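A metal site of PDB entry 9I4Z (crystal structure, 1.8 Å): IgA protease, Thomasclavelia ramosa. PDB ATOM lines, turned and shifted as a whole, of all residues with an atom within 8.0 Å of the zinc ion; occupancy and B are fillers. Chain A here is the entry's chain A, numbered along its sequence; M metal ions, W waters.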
ATOM      1  N   LEU A 223       2.183  31.121  27.894  1.00  0.00           N
ATOM      2  CA  LEU A 223       1.604  29.773  27.837  1.00  0.00           C
ATOM      3  C   LEU A 223       2.648  28.672  28.082  1.00  0.00           C
ATOM      4  O   LEU A 223       3.824  28.842  27.762  1.00  0.00           O
ATOM      5  CB  LEU A 223       0.927  29.557  26.491  1.00  0.00           C
ATOM      6  CG  LEU A 223      -0.092  30.632  26.098  1.00  0.00           C
ATOM      7  CD1 LEU A 223      -0.414  30.574  24.590  1.00  0.00           C
ATOM      8  CD2 LEU A 223      -1.377  30.552  26.951  1.00  0.00           C
ATOM      9  N   GLY A 224       2.193  27.547  28.595  1.00  0.00           N
ATOM     10  CA  GLY A 224       3.064  26.402  28.815  1.00  0.00           C
ATOM     11  C   GLY A 224       2.996  25.393  27.693  1.00  0.00           C
ATOM     12  O   GLY A 224       2.051  25.390  26.885  1.00  0.00           O
ATOM     13  N   ASP A 225       4.028  24.527  27.607  1.00  0.00           N
ATOM     14  CA  ASP A 225       4.059  23.423  26.650  1.00  0.00           C
ATOM     15  C   ASP A 225       2.925  22.445  27.009  1.00  0.00           C
ATOM     16  O   ASP A 225       2.864  21.945  28.140  1.00  0.00           O
ATOM     17  CB  ASP A 225       5.413  22.692  26.683  1.00  0.00           C
ATOM     18  CG  ASP A 225       6.503  23.426  25.928  1.00  0.00           C
ATOM     19  OD1 ASP A 225       7.612  23.528  26.458  1.00  0.00           O
ATOM     20  OD2 ASP A 225       6.234  23.889  24.806  1.00  0.00           O
ATOM     21  N   GLU A 226       2.025  22.186  26.064  1.00  0.00           N
ATOM     22  CA  GLU A 226       0.921  21.259  26.319  1.00  0.00           C
ATOM     23  C   GLU A 226       1.337  19.793  26.188  1.00  0.00           C
ATOM     24  O   GLU A 226       0.492  18.924  26.394  1.00  0.00           O
ATOM     25  CB  GLU A 226      -0.279  21.596  25.438  1.00  0.00           C
ATOM     26  CG  GLU A 226      -0.854  22.938  25.873  1.00  0.00           C
ATOM     27  CD  GLU A 226      -2.132  23.340  25.152  1.00  0.00           C
ATOM     28  OE1 GLU A 226      -2.698  22.486  24.430  1.00  0.00           O
ATOM     29  OE2 GLU A 226      -2.556  24.516  25.302  1.00  0.00           O
ATOM     30  N   ASN A 242      -2.657  27.550  30.853  1.00  0.00           N
ATOM     31  CA  ASN A 242      -3.328  26.633  29.925  1.00  0.00           C
ATOM     32  C   ASN A 242      -3.154  25.144  30.225  1.00  0.00           C
ATOM     33  O   ASN A 242      -3.544  24.320  29.408  1.00  0.00           O
ATOM     34  CB  ASN A 242      -2.822  26.901  28.499  1.00  0.00           C
ATOM     35  CG  ASN A 242      -1.324  26.693  28.354  1.00  0.00           C
ATOM     36  OD1 ASN A 242      -0.521  27.130  29.202  1.00  0.00           O
ATOM     37  ND2 ASN A 242      -0.926  26.011  27.307  1.00  0.00           N
ATOM     38  N   LEU A 243      -2.580  24.800  31.383  1.00  0.00           N
ATOM     39  CA  LEU A 243      -2.467  23.401  31.781  1.00  0.00           C
ATOM     40  C   LEU A 243      -3.231  23.180  33.097  1.00  0.00           C
ATOM     41  O   LEU A 243      -3.389  24.117  33.897  1.00  0.00           O
ATOM     42  CB  LEU A 243      -0.980  22.991  31.978  1.00  0.00           C
ATOM     43  CG  LEU A 243      -0.024  23.354  30.838  1.00  0.00           C
ATOM     44  CD1 LEU A 243       1.428  23.049  31.214  1.00  0.00           C
ATOM     45  CD2 LEU A 243      -0.383  22.639  29.580  1.00  0.00           C
ATOM     46  N   VAL A 276      -5.067  18.973  29.183  1.00  0.00           N
ATOM     47  CA  VAL A 276      -5.163  20.110  28.285  1.00  0.00           C
ATOM     48  C   VAL A 276      -6.630  20.343  27.931  1.00  0.00           C
ATOM     49  O   VAL A 276      -7.432  19.419  28.030  1.00  0.00           O
ATOM     50  CB  VAL A 276      -4.314  19.883  27.026  1.00  0.00           C
ATOM     51  CG1 VAL A 276      -2.826  19.830  27.389  1.00  0.00           C
ATOM     52  CG2 VAL A 276      -4.729  18.588  26.301  1.00  0.00           C
ATOM     53  N   SER A 277      -6.992  21.565  27.534  1.00  0.00           N
ATOM     54  CA  SER A 277      -8.403  21.874  27.222  1.00  0.00           C
ATOM     55  C   SER A 277      -8.823  21.332  25.847  1.00  0.00           C
ATOM     56  O   SER A 277     -10.015  21.220  25.570  1.00  0.00           O
ATOM     57  CB  SER A 277      -8.648  23.390  27.264  1.00  0.00           C
ATOM     58  OG  SER A 277      -8.003  24.053  26.195  1.00  0.00           O
ATOM     59  N   SER A 278      -7.843  21.087  24.959  1.00  0.00           N
ATOM     60  CA  SER A 278      -8.015  20.583  23.618  1.00  0.00           C
ATOM     61  C   SER A 278      -6.764  19.849  23.245  1.00  0.00           C
ATOM     62  O   SER A 278      -5.655  20.302  23.559  1.00  0.00           O
ATOM     63  CB  SER A 278      -8.272  21.724  22.638  1.00  0.00           C
ATOM     64  OG  SER A 278      -8.191  21.283  21.293  1.00  0.00           O
ATOM     65  N   TYR A 279      -6.919  18.723  22.557  1.00  0.00           N
ATOM     66  CA  TYR A 279      -5.751  17.966  22.097  1.00  0.00           C
ATOM     67  C   TYR A 279      -5.117  18.597  20.834  1.00  0.00           C
ATOM     68  O   TYR A 279      -3.969  18.280  20.499  1.00  0.00           O
ATOM     69  CB  TYR A 279      -6.187  16.528  21.824  1.00  0.00           C
ATOM     70  CG  TYR A 279      -5.011  15.600  21.687  1.00  0.00           C
ATOM     71  CD1 TYR A 279      -4.162  15.357  22.757  1.00  0.00           C
ATOM     72  CD2 TYR A 279      -4.715  15.015  20.465  1.00  0.00           C
ATOM     73  CE1 TYR A 279      -3.069  14.497  22.625  1.00  0.00           C
ATOM     74  CE2 TYR A 279      -3.623  14.178  20.316  1.00  0.00           C
ATOM     75  CZ  TYR A 279      -2.807  13.921  21.393  1.00  0.00           C
ATOM     76  OH  TYR A 279      -1.756  13.069  21.189  1.00  0.00           O
ATOM     77  N   GLU A 280      -5.822  19.515  20.165  1.00  0.00           N
ATOM     78  CA  GLU A 280      -5.341  20.110  18.938  1.00  0.00           C
ATOM     79  C   GLU A 280      -4.869  21.555  19.117  1.00  0.00           C
ATOM     80  O   GLU A 280      -5.531  22.487  18.650  1.00  0.00           O
ATOM     81  CB  GLU A 280      -6.461  20.025  17.876  1.00  0.00           C
ATOM     82  CG  GLU A 280      -6.874  18.580  17.617  1.00  0.00           C
ATOM     83  CD  GLU A 280      -8.010  18.456  16.626  1.00  0.00           C
ATOM     84  OE1 GLU A 280      -9.169  18.771  16.996  1.00  0.00           O
ATOM     85  OE2 GLU A 280      -7.751  18.045  15.470  1.00  0.00           O
ATOM     86  N   CYS A 281      -3.717  21.743  19.779  1.00  0.00           N
ATOM     87  CA  CYS A 281      -3.188  23.090  19.986  1.00  0.00           C
ATOM     88  C   CYS A 281      -1.747  23.151  19.550  1.00  0.00           C
ATOM     89  O   CYS A 281      -0.979  22.223  19.842  1.00  0.00           O
ATOM     90  CB  CYS A 281      -3.314  23.482  21.450  1.00  0.00           C
ATOM     91  SG  CYS A 281      -2.750  25.172  21.801  1.00  0.00           S
ATOM     92  N   ILE A 282      -1.334  24.325  19.048  1.00  0.00           N
ATOM     93  CA  ILE A 282       0.050  24.630  18.645  1.00  0.00           C
ATOM     94  C   ILE A 282       1.013  24.520  19.848  1.00  0.00           C
ATOM     95  O   ILE A 282       2.187  24.263  19.634  1.00  0.00           O
ATOM     96  CB  ILE A 282       0.111  26.064  18.038  1.00  0.00           C
ATOM     97  CG1 ILE A 282       1.420  26.267  17.234  1.00  0.00           C
ATOM     98  CG2 ILE A 282      -0.050  27.133  19.139  1.00  0.00           C
ATOM     99  CD1 ILE A 282       1.596  27.689  16.624  1.00  0.00           C
ATOM    100  N   MET A 283       0.502  24.690  21.099  1.00  0.00           N
ATOM    101  CA  MET A 283       1.377  24.585  22.253  1.00  0.00           C
ATOM    102  C   MET A 283       1.754  23.112  22.585  1.00  0.00           C
ATOM    103  O   MET A 283       2.666  22.876  23.376  1.00  0.00           O
ATOM    104  CB  MET A 283       0.804  25.342  23.448  1.00  0.00           C
ATOM    105  CG  MET A 283       0.656  26.885  23.172  1.00  0.00           C
ATOM    106  SD  MET A 283       2.172  27.681  22.535  1.00  0.00           S
ATOM    107  CE  MET A 283       3.343  27.379  23.928  1.00  0.00           C
ATOM    108  N   ARG A 284       1.086  22.134  21.940  1.00  0.00           N
ATOM    109  CA  ARG A 284       1.435  20.736  22.073  1.00  0.00           C
ATOM    110  C   ARG A 284       2.130  20.295  20.802  1.00  0.00           C
ATOM    111  O   ARG A 284       3.143  19.607  20.873  1.00  0.00           O
ATOM    112  CB  ARG A 284       0.171  19.883  22.323  1.00  0.00           C
ATOM    113  CG  ARG A 284       0.478  18.418  22.697  1.00  0.00           C
ATOM    114  CD  ARG A 284      -0.743  17.476  22.718  1.00  0.00           C
ATOM    115  NE  ARG A 284      -1.463  17.455  21.443  1.00  0.00           N
ATOM    116  CZ  ARG A 284      -1.095  16.751  20.379  1.00  0.00           C
ATOM    117  NH1 ARG A 284       0.002  16.011  20.406  1.00  0.00           N
ATOM    118  NH2 ARG A 284      -1.808  16.819  19.257  1.00  0.00           N
ATOM    119  N   GLN A 289      -3.502  25.225  15.398  1.00  0.00           N
ATOM    120  CA  GLN A 289      -3.774  26.607  15.768  1.00  0.00           C
ATOM    121  C   GLN A 289      -3.754  26.712  17.304  1.00  0.00           C
ATOM    122  O   GLN A 289      -3.667  25.679  17.983  1.00  0.00           O
ATOM    123  CB  GLN A 289      -5.153  27.024  15.226  1.00  0.00           C
ATOM    124  CG  GLN A 289      -5.228  27.000  13.711  1.00  0.00           C
ATOM    125  CD  GLN A 289      -4.630  28.252  13.121  1.00  0.00           C
ATOM    126  OE1 GLN A 289      -4.750  29.360  13.680  1.00  0.00           O
ATOM    127  NE2 GLN A 289      -3.965  28.107  11.980  1.00  0.00           N
ATOM    128  N   PHE A 290      -3.870  27.933  17.853  1.00  0.00           N
ATOM    129  CA  PHE A 290      -4.014  28.093  19.308  1.00  0.00           C
ATOM    130  C   PHE A 290      -5.433  27.631  19.710  1.00  0.00           C
ATOM    131  O   PHE A 290      -6.393  27.964  19.026  1.00  0.00           O
ATOM    132  CB  PHE A 290      -3.764  29.555  19.752  1.00  0.00           C
ATOM    133  CG  PHE A 290      -2.318  29.966  19.670  1.00  0.00           C
ATOM    134  CD1 PHE A 290      -1.791  30.481  18.498  1.00  0.00           C
ATOM    135  CD2 PHE A 290      -1.478  29.825  20.763  1.00  0.00           C
ATOM    136  CE1 PHE A 290      -0.441  30.819  18.417  1.00  0.00           C
ATOM    137  CE2 PHE A 290      -0.138  30.175  20.677  1.00  0.00           C
ATOM    138  CZ  PHE A 290       0.373  30.692  19.521  1.00  0.00           C
ATOM    139  N   CYS A 291      -5.530  26.838  20.772  1.00  0.00           N
ATOM    140  CA  CYS A 291      -6.836  26.364  21.310  1.00  0.00           C
ATOM    141  C   CYS A 291      -7.634  27.554  21.892  1.00  0.00           C
ATOM    142  O   CYS A 291      -7.087  28.631  22.020  1.00  0.00           O
ATOM    143  CB  CYS A 291      -6.619  25.254  22.349  1.00  0.00           C
ATOM    144  SG  CYS A 291      -5.946  25.815  23.955  1.00  0.00           S
ATOM    145  N   GLU A 292      -8.924  27.346  22.278  1.00  0.00           N
ATOM    146  CA  GLU A 292      -9.732  28.437  22.843  1.00  0.00           C
ATOM    147  C   GLU A 292      -9.165  28.959  24.154  1.00  0.00           C
ATOM    148  O   GLU A 292      -9.240  30.154  24.401  1.00  0.00           O
ATOM    149  CB  GLU A 292     -11.203  28.001  23.064  1.00  0.00           C
ATOM    150  CG  GLU A 292     -11.918  27.641  21.774  1.00  0.00           C
ATOM    151  CD  GLU A 292     -11.887  28.689  20.675  1.00  0.00           C
ATOM    152  OE1 GLU A 292     -12.044  29.901  20.991  1.00  0.00           O
ATOM    153  OE2 GLU A 292     -11.724  28.298  19.508  1.00  0.00           O
ATOM    154  N   VAL A 293      -8.587  28.091  25.005  1.00  0.00           N
ATOM    155  CA  VAL A 293      -8.028  28.557  26.285  1.00  0.00           C
ATOM    156  C   VAL A 293      -6.796  29.422  25.993  1.00  0.00           C
ATOM    157  O   VAL A 293      -6.673  30.521  26.558  1.00  0.00           O
ATOM    158  CB  VAL A 293      -7.701  27.375  27.238  1.00  0.00           C
ATOM    159  CG1 VAL A 293      -6.767  27.806  28.377  1.00  0.00           C
ATOM    160  CG2 VAL A 293      -9.010  26.776  27.794  1.00  0.00           C
ATOM    161  N   CYS A 294      -5.910  28.969  25.112  1.00  0.00           N
ATOM    162  CA  CYS A 294      -4.736  29.782  24.762  1.00  0.00           C
ATOM    163  C   CYS A 294      -5.135  31.091  24.097  1.00  0.00           C
ATOM    164  O   CYS A 294      -4.480  32.110  24.331  1.00  0.00           O
ATOM    165  CB  CYS A 294      -3.746  28.994  23.911  1.00  0.00           C
ATOM    166  SG  CYS A 294      -2.854  27.731  24.851  1.00  0.00           S
ATOM    167  N   ARG A 295      -6.193  31.072  23.274  1.00  0.00           N
ATOM    168  CA  ARG A 295      -6.668  32.293  22.613  1.00  0.00           C
ATOM    169  C   ARG A 295      -7.164  33.282  23.664  1.00  0.00           C
ATOM    170  O   ARG A 295      -6.764  34.441  23.647  1.00  0.00           O
ATOM    171  CB  ARG A 295      -7.773  31.958  21.624  1.00  0.00           C
ATOM    172  CG  ARG A 295      -7.213  31.405  20.315  1.00  0.00           C
ATOM    173  CD  ARG A 295      -8.334  30.970  19.396  1.00  0.00           C
ATOM    174  NE  ARG A 295      -7.824  30.298  18.193  1.00  0.00           N
ATOM    175  CZ  ARG A 295      -8.350  30.444  16.983  1.00  0.00           C
ATOM    176  NH1 ARG A 295      -9.382  31.258  16.784  1.00  0.00           N
ATOM    177  NH2 ARG A 295      -7.829  29.799  15.941  1.00  0.00           N
HETATM  178 ZN    ZN M   1      -3.596  25.691  23.888  1.00  0.00          ZN
HETATM  179  O   HOH W   1      -5.302  22.874  24.809  1.00  0.00           O
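ND2 of Asn 242 sits close to SG of Cys 294 (3.6 Å).
The side-chain sulfur of Cys 291 sits close to the side-chain hydroxyl of Ser 277, 3.5 Å away.
ND2 of Asn 242 sits close to OE2 of Glu 226, at 3.0 Å.
The side-chain sulfur of Cys 281 lies close to the backbone NH of Met 283 (3.4 Å).
The side-chain sulfur (SG) of Cys 291 lies close to the backbone NH (N) of Val 293 (3.6 Å).
N of Glu 226 sits at hydrogen-bond distance from O of Met 283.
Of the 22 residues printed, 4 come within 4 Å of the zinc ion.
The nearest printed residue that does not touch the zinc ion is Asn 242 (4.3 Å).
The zinc ion is bound by OE2 of Glu 226 (2.1 Å), SG of Cys 281 (2.3 Å), SG of Cys 291 (2.4 Å) and SG of Cys 294 (2.4 Å).
The zinc ion has four donor atoms within binding distance.
Water W1 lies within hydrogen-bond range of the side-chain carboxylate of Glu 226, the backbone carbonyl oxygen of Ser 278 and the side-chain hydroxyl of Ser 277.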
